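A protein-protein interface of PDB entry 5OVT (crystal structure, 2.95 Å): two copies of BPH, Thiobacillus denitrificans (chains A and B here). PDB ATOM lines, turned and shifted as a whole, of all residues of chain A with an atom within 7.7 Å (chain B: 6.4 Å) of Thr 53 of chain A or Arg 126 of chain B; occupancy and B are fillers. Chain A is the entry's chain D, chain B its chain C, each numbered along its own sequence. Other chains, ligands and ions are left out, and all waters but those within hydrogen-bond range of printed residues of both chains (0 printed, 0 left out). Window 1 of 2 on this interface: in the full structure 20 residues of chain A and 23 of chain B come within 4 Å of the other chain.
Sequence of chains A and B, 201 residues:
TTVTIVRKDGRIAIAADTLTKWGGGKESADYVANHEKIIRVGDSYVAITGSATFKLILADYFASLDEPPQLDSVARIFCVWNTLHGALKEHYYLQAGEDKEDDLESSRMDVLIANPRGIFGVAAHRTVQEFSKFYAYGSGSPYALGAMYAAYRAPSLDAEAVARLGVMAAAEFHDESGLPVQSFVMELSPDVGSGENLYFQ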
ATOM      1  N   ILE A  48      37.938 -13.289  -1.452  1.00  0.00           N
ATOM      2  CA  ILE A  48      37.338 -14.071  -0.399  1.00  0.00           C
ATOM      3  C   ILE A  48      37.509 -15.592  -0.568  1.00  0.00           C
ATOM      4  O   ILE A  48      37.310 -16.121  -1.655  1.00  0.00           O
ATOM      5  CB  ILE A  48      35.866 -13.732  -0.333  1.00  0.00           C
ATOM      6  CG1 ILE A  48      35.723 -12.228  -0.113  1.00  0.00           C
ATOM      7  CG2 ILE A  48      35.197 -14.465   0.821  1.00  0.00           C
ATOM      8  CD1 ILE A  48      34.315 -11.698  -0.379  1.00  0.00           C
ATOM      9  N   GLY A  50      36.377 -19.402   1.484  1.00  0.00           N
ATOM     10  CA  GLY A  50      35.399 -19.840   2.447  1.00  0.00           C
ATOM     11  C   GLY A  50      34.109 -20.135   1.774  1.00  0.00           C
ATOM     12  O   GLY A  50      34.051 -20.242   0.574  1.00  0.00           O
ATOM     13  N   SER A  51      33.052 -20.247   2.543  1.00  0.00           N
ATOM     14  CA  SER A  51      31.741 -20.380   1.960  1.00  0.00           C
ATOM     15  C   SER A  51      31.443 -19.303   0.930  1.00  0.00           C
ATOM     16  O   SER A  51      31.726 -18.140   1.119  1.00  0.00           O
ATOM     17  CB  SER A  51      30.678 -20.340   3.038  1.00  0.00           C
ATOM     18  OG  SER A  51      29.407 -20.152   2.439  1.00  0.00           O
ATOM     19  N   ALA A  52      30.858 -19.699  -0.182  1.00  0.00           N
ATOM     20  CA  ALA A  52      30.430 -18.737  -1.209  1.00  0.00           C
ATOM     21  C   ALA A  52      29.461 -17.689  -0.716  1.00  0.00           C
ATOM     22  O   ALA A  52      29.391 -16.602  -1.277  1.00  0.00           O
ATOM     23  CB  ALA A  52      29.813 -19.474  -2.372  1.00  0.00           C
ATOM     24  N   THR A  53      28.715 -18.002   0.331  1.00  0.00           N
ATOM     25  CA  THR A  53      27.824 -17.019   0.916  1.00  0.00           C
ATOM     26  C   THR A  53      28.513 -15.741   1.427  1.00  0.00           C
ATOM     27  O   THR A  53      27.934 -14.670   1.374  1.00  0.00           O
ATOM     28  CB  THR A  53      27.017 -17.614   2.053  1.00  0.00           C
ATOM     29  OG1 THR A  53      26.376 -18.798   1.598  1.00  0.00           O
ATOM     30  CG2 THR A  53      25.955 -16.670   2.498  1.00  0.00           C
ATOM     31  N   PHE A  54      29.774 -15.818   1.807  1.00  0.00           N
ATOM     32  CA  PHE A  54      30.437 -14.647   2.342  1.00  0.00           C
ATOM     33  C   PHE A  54      30.629 -13.525   1.339  1.00  0.00           C
ATOM     34  O   PHE A  54      30.559 -12.357   1.719  1.00  0.00           O
ATOM     35  CB  PHE A  54      31.766 -15.024   2.988  1.00  0.00           C
ATOM     36  CG  PHE A  54      31.614 -15.761   4.288  1.00  0.00           C
ATOM     37  CD1 PHE A  54      31.069 -15.150   5.395  1.00  0.00           C
ATOM     38  CD2 PHE A  54      31.993 -17.066   4.388  1.00  0.00           C
ATOM     39  CE1 PHE A  54      30.884 -15.837   6.585  1.00  0.00           C
ATOM     40  CE2 PHE A  54      31.805 -17.769   5.574  1.00  0.00           C
ATOM     41  CZ  PHE A  54      31.246 -17.158   6.675  1.00  0.00           C
ATOM     42  N   LYS A  55      30.866 -13.852   0.070  1.00  0.00           N
ATOM     43  CA  LYS A  55      30.855 -12.809  -1.028  1.00  0.00           C
ATOM     44  C   LYS A  55      29.638 -11.899  -0.837  1.00  0.00           C
ATOM     45  O   LYS A  55      29.764 -10.697  -0.730  1.00  0.00           O
ATOM     46  CB  LYS A  55      30.873 -13.488  -2.427  1.00  0.00           C
ATOM     47  CG  LYS A  55      30.793 -12.586  -3.652  1.00  0.00           C
ATOM     48  CD  LYS A  55      30.761 -13.289  -5.047  1.00  0.00           C
ATOM     49  CE  LYS A  55      29.952 -14.617  -5.161  1.00  0.00           C
ATOM     50  NZ  LYS A  55      30.694 -15.948  -5.213  1.00  0.00           N
ATOM     51  N   LEU A  56      28.456 -12.489  -0.711  1.00  0.00           N
ATOM     52  CA  LEU A  56      27.237 -11.698  -0.636  1.00  0.00           C
ATOM     53  C   LEU A  56      27.046 -11.002   0.691  1.00  0.00           C
ATOM     54  O   LEU A  56      26.466  -9.923   0.746  1.00  0.00           O
ATOM     55  CB  LEU A  56      26.025 -12.585  -0.885  1.00  0.00           C
ATOM     56  CG  LEU A  56      26.119 -13.337  -2.214  1.00  0.00           C
ATOM     57  CD1 LEU A  56      25.388 -14.680  -2.137  1.00  0.00           C
ATOM     58  CD2 LEU A  56      25.622 -12.395  -3.313  1.00  0.00           C
ATOM     59  N   ILE A  57      27.444 -11.655   1.763  1.00  0.00           N
ATOM     60  CA  ILE A  57      27.336 -11.062   3.061  1.00  0.00           C
ATOM     61  C   ILE A  57      28.184  -9.809   3.177  1.00  0.00           C
ATOM     62  O   ILE A  57      27.725  -8.780   3.650  1.00  0.00           O
ATOM     63  CB  ILE A  57      27.777 -12.042   4.150  1.00  0.00           C
ATOM     64  CG1 ILE A  57      26.763 -13.179   4.255  1.00  0.00           C
ATOM     65  CG2 ILE A  57      27.840 -11.329   5.489  1.00  0.00           C
ATOM     66  CD1 ILE A  57      27.165 -14.302   5.182  1.00  0.00           C
ATOM     67  N   LEU A  58      29.434  -9.902   2.788  1.00  0.00           N
ATOM     68  CA  LEU A  58      30.271  -8.725   2.846  1.00  0.00           C
ATOM     69  C   LEU A  58      29.777  -7.592   1.952  1.00  0.00           C
ATOM     70  O   LEU A  58      29.764  -6.437   2.366  1.00  0.00           O
ATOM     71  CB  LEU A  58      31.695  -9.048   2.465  1.00  0.00           C
ATOM     72  CG  LEU A  58      32.442 -10.020   3.376  1.00  0.00           C
ATOM     73  CD1 LEU A  58      33.927  -9.913   3.095  1.00  0.00           C
ATOM     74  CD2 LEU A  58      32.232  -9.791   4.849  1.00  0.00           C
ATOM     75  N   ALA A  59      29.337  -7.922   0.758  1.00  0.00           N
ATOM     76  CA  ALA A  59      28.781  -6.910  -0.105  1.00  0.00           C
ATOM     77  C   ALA A  59      27.590  -6.169   0.577  1.00  0.00           C
ATOM     78  O   ALA A  59      27.570  -4.939   0.603  1.00  0.00           O
ATOM     79  CB  ALA A  59      28.373  -7.528  -1.428  1.00  0.00           C
ATOM     80  N   HIS A  91      23.288 -10.656  12.607  1.00  0.00           N
ATOM     81  CA  HIS A  91      22.393 -10.457  11.426  1.00  0.00           C
ATOM     82  C   HIS A  91      22.484 -11.574  10.409  1.00  0.00           C
ATOM     83  O   HIS A  91      21.544 -11.775   9.651  1.00  0.00           O
ATOM     84  CB  HIS A  91      22.643  -9.089  10.690  1.00  0.00           C
ATOM     85  CG  HIS A  91      21.595  -8.685   9.661  1.00  0.00           C
ATOM     86  ND1 HIS A  91      20.312  -8.308   9.996  1.00  0.00           N
ATOM     87  CD2 HIS A  91      21.686  -8.505   8.321  1.00  0.00           C
ATOM     88  CE1 HIS A  91      19.643  -7.980   8.907  1.00  0.00           C
ATOM     89  NE2 HIS A  91      20.454  -8.092   7.874  1.00  0.00           N
ATOM     90  N   TYR A  92      23.617 -12.268  10.332  1.00  0.00           N
ATOM     91  CA  TYR A  92      23.866 -13.187   9.187  1.00  0.00           C
ATOM     92  C   TYR A  92      23.971 -14.679   9.517  1.00  0.00           C
ATOM     93  O   TYR A  92      24.261 -15.495   8.600  1.00  0.00           O
ATOM     94  CB  TYR A  92      25.108 -12.740   8.422  1.00  0.00           C
ATOM     95  CG  TYR A  92      24.985 -11.366   7.777  1.00  0.00           C
ATOM     96  CD1 TYR A  92      24.221 -11.179   6.647  1.00  0.00           C
ATOM     97  CD2 TYR A  92      25.656 -10.261   8.294  1.00  0.00           C
ATOM     98  CE1 TYR A  92      24.147  -9.922   6.049  1.00  0.00           C
ATOM     99  CE2 TYR A  92      25.567  -9.028   7.709  1.00  0.00           C
ATOM    100  CZ  TYR A  92      24.820  -8.858   6.594  1.00  0.00           C
ATOM    101  OH  TYR A  92      24.767  -7.622   5.993  1.00  0.00           O
ATOM    102  N   TYR A  93      23.703 -15.008  10.784  1.00  0.00           N
ATOM    103  CA  TYR A  93      23.558 -16.372  11.246  1.00  0.00           C
ATOM    104  C   TYR A  93      24.820 -17.214  11.204  1.00  0.00           C
ATOM    105  O   TYR A  93      24.747 -18.421  10.990  1.00  0.00           O
ATOM    106  CB  TYR A  93      22.422 -17.106  10.517  1.00  0.00           C
ATOM    107  CG  TYR A  93      21.134 -16.344  10.473  1.00  0.00           C
ATOM    108  CD1 TYR A  93      20.364 -16.198  11.612  1.00  0.00           C
ATOM    109  CD2 TYR A  93      20.711 -15.720   9.300  1.00  0.00           C
ATOM    110  CE1 TYR A  93      19.199 -15.449  11.598  1.00  0.00           C
ATOM    111  CE2 TYR A  93      19.557 -14.967   9.263  1.00  0.00           C
ATOM    112  CZ  TYR A  93      18.805 -14.838  10.417  1.00  0.00           C
ATOM    113  OH  TYR A  93      17.655 -14.104  10.367  1.00  0.00           O
ATOM    114  N   LEU A  94      25.979 -16.605  11.448  1.00  0.00           N
ATOM    115  CA  LEU A  94      27.231 -17.352  11.742  1.00  0.00           C
ATOM    116  C   LEU A  94      27.114 -18.009  13.083  1.00  0.00           C
ATOM    117  O   LEU A  94      26.502 -17.386  13.949  1.00  0.00           O
ATOM    118  CB  LEU A  94      28.365 -16.355  11.845  1.00  0.00           C
ATOM    119  CG  LEU A  94      29.758 -16.933  11.948  1.00  0.00           C
ATOM    120  CD1 LEU A  94      30.177 -17.480  10.609  1.00  0.00           C
ATOM    121  CD2 LEU A  94      30.738 -15.865  12.351  1.00  0.00           C
ATOM    122  N   PHE B  78      19.252 -12.750  -1.958  1.00  0.00           N
ATOM    123  CA  PHE B  78      19.954 -12.863  -0.715  1.00  0.00           C
ATOM    124  C   PHE B  78      19.238 -12.227   0.460  1.00  0.00           C
ATOM    125  O   PHE B  78      19.124 -12.843   1.505  1.00  0.00           O
ATOM    126  CB  PHE B  78      21.356 -12.305  -0.835  1.00  0.00           C
ATOM    127  CG  PHE B  78      22.115 -12.402   0.415  1.00  0.00           C
ATOM    128  CD1 PHE B  78      22.511 -13.639   0.900  1.00  0.00           C
ATOM    129  CD2 PHE B  78      22.353 -11.301   1.170  1.00  0.00           C
ATOM    130  CE1 PHE B  78      23.174 -13.757   2.098  1.00  0.00           C
ATOM    131  CE2 PHE B  78      23.049 -11.407   2.360  1.00  0.00           C
ATOM    132  CZ  PHE B  78      23.449 -12.635   2.827  1.00  0.00           C
ATOM    133  N   TRP B  81      16.133 -14.142   1.450  1.00  0.00           N
ATOM    134  CA  TRP B  81      16.429 -15.399   2.144  1.00  0.00           C
ATOM    135  C   TRP B  81      17.008 -15.217   3.544  1.00  0.00           C
ATOM    136  O   TRP B  81      16.747 -16.011   4.447  1.00  0.00           O
ATOM    137  CB  TRP B  81      17.304 -16.314   1.275  1.00  0.00           C
ATOM    138  CG  TRP B  81      16.579 -17.558   0.860  1.00  0.00           C
ATOM    139  CD1 TRP B  81      16.779 -18.777   1.357  1.00  0.00           C
ATOM    140  CD2 TRP B  81      15.520 -17.660  -0.071  1.00  0.00           C
ATOM    141  NE1 TRP B  81      15.915 -19.652   0.775  1.00  0.00           N
ATOM    142  CE2 TRP B  81      15.130 -18.980  -0.111  1.00  0.00           C
ATOM    143  CE3 TRP B  81      14.844 -16.735  -0.860  1.00  0.00           C
ATOM    144  CZ2 TRP B  81      14.112 -19.434  -0.908  1.00  0.00           C
ATOM    145  CZ3 TRP B  81      13.819 -17.183  -1.675  1.00  0.00           C
ATOM    146  CH2 TRP B  81      13.472 -18.522  -1.688  1.00  0.00           C
ATOM    147  N   ASN B  82      17.809 -14.176   3.729  1.00  0.00           N
ATOM    148  CA  ASN B  82      18.336 -13.914   5.061  1.00  0.00           C
ATOM    149  C   ASN B  82      17.210 -13.588   6.047  1.00  0.00           C
ATOM    150  O   ASN B  82      17.269 -13.961   7.217  1.00  0.00           O
ATOM    151  CB  ASN B  82      19.384 -12.817   5.017  1.00  0.00           C
ATOM    152  CG  ASN B  82      20.432 -12.999   6.039  1.00  0.00           C
ATOM    153  OD1 ASN B  82      21.181 -14.037   6.065  1.00  0.00           O
ATOM    154  ND2 ASN B  82      20.532 -12.021   6.902  1.00  0.00           N
ATOM    155  N   THR B  83      16.176 -12.923   5.565  1.00  0.00           N
ATOM    156  CA  THR B  83      15.040 -12.584   6.410  1.00  0.00           C
ATOM    157  C   THR B  83      14.218 -13.821   6.690  1.00  0.00           C
ATOM    158  O   THR B  83      13.835 -14.103   7.854  1.00  0.00           O
ATOM    159  CB  THR B  83      14.114 -11.546   5.721  1.00  0.00           C
ATOM    160  OG1 THR B  83      14.810 -10.323   5.599  1.00  0.00           O
ATOM    161  CG2 THR B  83      12.850 -11.327   6.509  1.00  0.00           C
ATOM    162  N   HIS B  85      15.122 -16.838   6.742  1.00  0.00           N
ATOM    163  CA  HIS B  85      15.734 -17.758   7.642  1.00  0.00           C
ATOM    164  C   HIS B  85      15.319 -17.434   9.067  1.00  0.00           C
ATOM    165  O   HIS B  85      15.006 -18.338   9.863  1.00  0.00           O
ATOM    166  CB  HIS B  85      17.230 -17.684   7.527  1.00  0.00           C
ATOM    167  CG  HIS B  85      17.916 -18.680   8.382  1.00  0.00           C
ATOM    168  ND1 HIS B  85      17.992 -20.006   8.049  1.00  0.00           N
ATOM    169  CD2 HIS B  85      18.484 -18.566   9.606  1.00  0.00           C
ATOM    170  CE1 HIS B  85      18.613 -20.672   9.014  1.00  0.00           C
ATOM    171  NE2 HIS B  85      18.903 -19.824   9.981  1.00  0.00           N
ATOM    172  N   LEU B 104      28.029 -21.123   8.924  1.00  0.00           N
ATOM    173  CA  LEU B 104      26.703 -20.487   8.936  1.00  0.00           C
ATOM    174  C   LEU B 104      25.551 -21.465   9.191  1.00  0.00           C
ATOM    175  O   LEU B 104      25.633 -22.577   8.740  1.00  0.00           O
ATOM    176  CB  LEU B 104      26.413 -19.861   7.568  1.00  0.00           C
ATOM    177  CG  LEU B 104      27.435 -18.840   7.102  1.00  0.00           C
ATOM    178  CD1 LEU B 104      27.220 -18.586   5.647  1.00  0.00           C
ATOM    179  CD2 LEU B 104      27.312 -17.556   7.901  1.00  0.00           C
ATOM    180  N   GLU B 105      24.439 -21.020   9.810  1.00  0.00           N
ATOM    181  CA  GLU B 105      23.262 -21.887  10.040  1.00  0.00           C
ATOM    182  C   GLU B 105      22.685 -22.344   8.741  1.00  0.00           C
ATOM    183  O   GLU B 105      22.917 -21.707   7.811  1.00  0.00           O
ATOM    184  CB  GLU B 105      22.175 -21.145  10.740  1.00  0.00           C
ATOM    185  CG  GLU B 105      22.527 -20.903  12.180  1.00  0.00           C
ATOM    186  CD  GLU B 105      21.451 -20.173  12.956  1.00  0.00           C
ATOM    187  OE1 GLU B 105      20.302 -19.999  12.494  1.00  0.00           O
ATOM    188  OE2 GLU B 105      21.782 -19.734  14.061  1.00  0.00           O
ATOM    189  N   SER B 106      21.971 -23.461   8.672  1.00  0.00           N
ATOM    190  CA  SER B 106      21.432 -23.953   7.413  1.00  0.00           C
ATOM    191  C   SER B 106      19.941 -23.728   7.385  1.00  0.00           C
ATOM    192  O   SER B 106      19.261 -23.873   8.382  1.00  0.00           O
ATOM    193  CB  SER B 106      21.726 -25.420   7.258  1.00  0.00           C
ATOM    194  OG  SER B 106      21.193 -25.978   6.080  1.00  0.00           O
ATOM    195  N   SER B 107      19.414 -23.340   6.226  1.00  0.00           N
ATOM    196  CA  SER B 107      17.965 -23.215   6.056  1.00  0.00           C
ATOM    197  C   SER B 107      17.369 -24.543   5.645  1.00  0.00           C
ATOM    198  O   SER B 107      16.163 -24.696   5.590  1.00  0.00           O
ATOM    199  CB  SER B 107      17.664 -22.109   5.069  1.00  0.00           C
ATOM    200  OG  SER B 107      18.214 -20.888   5.549  1.00  0.00           O
ATOM    201  N   VAL B 122      19.268 -20.943  -4.691  1.00  0.00           N
ATOM    202  CA  VAL B 122      19.698 -20.679  -3.322  1.00  0.00           C
ATOM    203  C   VAL B 122      19.907 -21.984  -2.591  1.00  0.00           C
ATOM    204  O   VAL B 122      18.985 -22.803  -2.450  1.00  0.00           O
ATOM    205  CB  VAL B 122      18.664 -19.908  -2.541  1.00  0.00           C
ATOM    206  CG1 VAL B 122      19.268 -19.311  -1.300  1.00  0.00           C
ATOM    207  CG2 VAL B 122      18.128 -18.797  -3.390  1.00  0.00           C
ATOM    208  N   ALA B 123      21.121 -22.179  -2.130  1.00  0.00           N
ATOM    209  CA  ALA B 123      21.445 -23.396  -1.444  1.00  0.00           C
ATOM    210  C   ALA B 123      21.265 -23.204   0.043  1.00  0.00           C
ATOM    211  O   ALA B 123      20.928 -22.139   0.522  1.00  0.00           O
ATOM    212  CB  ALA B 123      22.848 -23.799  -1.764  1.00  0.00           C
ATOM    213  N   ALA B 124      21.409 -24.280   0.790  1.00  0.00           N
ATOM    214  CA  ALA B 124      20.952 -24.276   2.176  1.00  0.00           C
ATOM    215  C   ALA B 124      21.683 -23.324   3.041  1.00  0.00           C
ATOM    216  O   ALA B 124      21.121 -22.913   4.046  1.00  0.00           O
ATOM    217  CB  ALA B 124      21.010 -25.667   2.751  1.00  0.00           C
ATOM    218  N   HIS B 125      22.906 -22.951   2.694  1.00  0.00           N
ATOM    219  CA  HIS B 125      23.563 -21.945   3.517  1.00  0.00           C
ATOM    220  C   HIS B 125      23.488 -20.569   2.926  1.00  0.00           C
ATOM    221  O   HIS B 125      24.370 -19.750   3.122  1.00  0.00           O
ATOM    222  CB  HIS B 125      24.989 -22.331   3.843  1.00  0.00           C
ATOM    223  CG  HIS B 125      25.089 -23.596   4.631  1.00  0.00           C
ATOM    224  ND1 HIS B 125      25.013 -24.847   4.057  1.00  0.00           N
ATOM    225  CD2 HIS B 125      25.193 -23.808   5.955  1.00  0.00           C
ATOM    226  CE1 HIS B 125      25.095 -25.776   4.989  1.00  0.00           C
ATOM    227  NE2 HIS B 125      25.187 -25.172   6.154  1.00  0.00           N
ATOM    228  N   ARG B 126      22.397 -20.317   2.219  1.00  0.00           N
ATOM    229  CA  ARG B 126      22.117 -19.022   1.573  1.00  0.00           C
ATOM    230  C   ARG B 126      23.117 -18.545   0.516  1.00  0.00           C
ATOM    231  O   ARG B 126      23.285 -17.365   0.271  1.00  0.00           O
ATOM    232  CB  ARG B 126      21.882 -17.977   2.641  1.00  0.00           C
ATOM    233  CG  ARG B 126      20.460 -18.023   3.204  1.00  0.00           C
ATOM    234  CD  ARG B 126      20.418 -17.513   4.623  1.00  0.00           C
ATOM    235  NE  ARG B 126      20.680 -18.698   5.408  1.00  0.00           N
ATOM    236  CZ  ARG B 126      21.663 -18.836   6.261  1.00  0.00           C
ATOM    237  NH1 ARG B 126      22.541 -17.852   6.541  1.00  0.00           N
ATOM    238  NH2 ARG B 126      21.728 -19.985   6.867  1.00  0.00           N
ATOM    239  N   THR B 127      23.773 -19.493  -0.122  1.00  0.00           N
ATOM    240  CA  THR B 127      24.564 -19.164  -1.264  1.00  0.00           C
ATOM    241  C   THR B 127      23.641 -18.975  -2.434  1.00  0.00           C
ATOM    242  O   THR B 127      22.970 -19.904  -2.832  1.00  0.00           O
ATOM    243  CB  THR B 127      25.556 -20.272  -1.603  1.00  0.00           C
ATOM    244  OG1 THR B 127      26.497 -20.344  -0.553  1.00  0.00           O
ATOM    245  CG2 THR B 127      26.293 -19.951  -2.893  1.00  0.00           C
ATOM    246  N   VAL B 128      23.598 -17.760  -2.949  1.00  0.00           N
ATOM    247  CA  VAL B 128      22.716 -17.425  -4.043  1.00  0.00           C
ATOM    248  C   VAL B 128      23.537 -17.380  -5.301  1.00  0.00           C
ATOM    249  O   VAL B 128      24.505 -16.669  -5.374  1.00  0.00           O
ATOM    250  CB  VAL B 128      22.061 -16.041  -3.848  1.00  0.00           C
ATOM    251  CG1 VAL B 128      21.177 -15.687  -5.016  1.00  0.00           C
ATOM    252  CG2 VAL B 128      21.260 -16.001  -2.571  1.00  0.00           C
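No position is printed for both chains.
The backbone carbonyl oxygen (O) of Asn 82 of chain B sits at hydrogen-bond distance from the side-chain hydroxyl (OH) of Tyr 93 of chain A (3.2 Å).
OG1 of Thr 127 of chain B is in hydrogen-bond range of OG1 of Thr 53 of chain A (2.7 Å).
O of His 125 of chain B lies within hydrogen-bond range of OG1 of Thr 53 of chain A (2.7 Å).
The backbone carbonyl oxygen of Tyr 93 of chain A is in hydrogen-bond range of the backbone NH of Glu 105 of chain B (2.9 Å).
The backbone carbonyl oxygen (O) of His 91 of chain A is in hydrogen-bond range of the side-chain amide nitrogen (ND2) of Asn 82 of chain B.
Of the 16 printed residues of chain B, 9 touch a printed residue of chain A.
Hydrophobic or aromatic side chains of chain B within 4 Å of the printed part of chain A: Phe 78, His 85, Leu 104 and Val 128.
Among the printed residues, 17 pairs touch across the chains.
Among the printed residues, no Asp or Glu carboxylate lies within 4 Å of a Lys or Arg side-chain nitrogen of the other chain.
CG2 of Thr 127 of chain B touches CB of Ala 52 of chain A, at 3.6 Å.
Thr 53 of chain A touches Leu 104 of chain B.
Thr 53 of chain A touches Arg 126 of chain B (OG1 to C, 3.4 Å).
Ile 57 of chain A touches Phe 78 of chain B (CG1 to CZ, 3.6 Å).
Tyr 92 of chain A touches Asn 82 of chain B (CD1 to ND2, 3.8 Å).
Tyr 92 of chain A touches Leu 104 of chain B (O to CD2, 3.7 Å).
His 85 of chain B touches Tyr 93 of chain A (CD2 to CG, 3.6 Å).
Tyr 93 of chain A touches Leu 104 of chain B.
CD2 of Tyr 93 of chain A touches NH1 of Arg 126 of chain B (3.9 Å).
CA of Leu 94 of chain A touches CD2 of Leu 104 of chain B, 3.8 Å away.
Arg 126 of chain B touches just these residues of chain A: Thr 53, Tyr 92 and Tyr 93.
Printed residues of chain A within 4 Å of Asn 82 of chain B: His 91 (2.9 Å), Tyr 92 (3.8 Å) and Tyr 93 (3.2 Å).
Of the printed residues of chain A, His 85 of chain B touches Tyr 93.
Of the printed residues of chain A, Glu 105 of chain B touches Tyr 93.
The nearest residue of chain B that does not touch Thr 53 of chain A is Phe 78 of chain B (4.05 Å).
The nearest residue of chain A that does not touch Arg 126 of chain B is Leu 56 of chain A (4.2 Å).
The nearest printed residue of chain B that does not touch Ala 52 of chain A is Val 128 of chain B (6.1 Å).
A ring nitrogen (NE2) of His 85 of chain B is in hydrogen-bond range of the side-chain carboxylate of Glu 105 of chain B (2.9 Å).
The side-chain hydroxyl (OG) of Ser 51 of chain A lies close to the backbone NH (N) of Thr 53 of chain A (3.1 Å).
The side-chain hydroxyl (OG) of Ser 107 of chain B is in hydrogen-bond range of the guanidinium group (NE) of Arg 126 of chain B.
A ring nitrogen (ND1) of His 85 of chain B lies within hydrogen-bond range of the side-chain hydroxyl (OG) of Ser 107 of chain B, at 2.7 Å.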
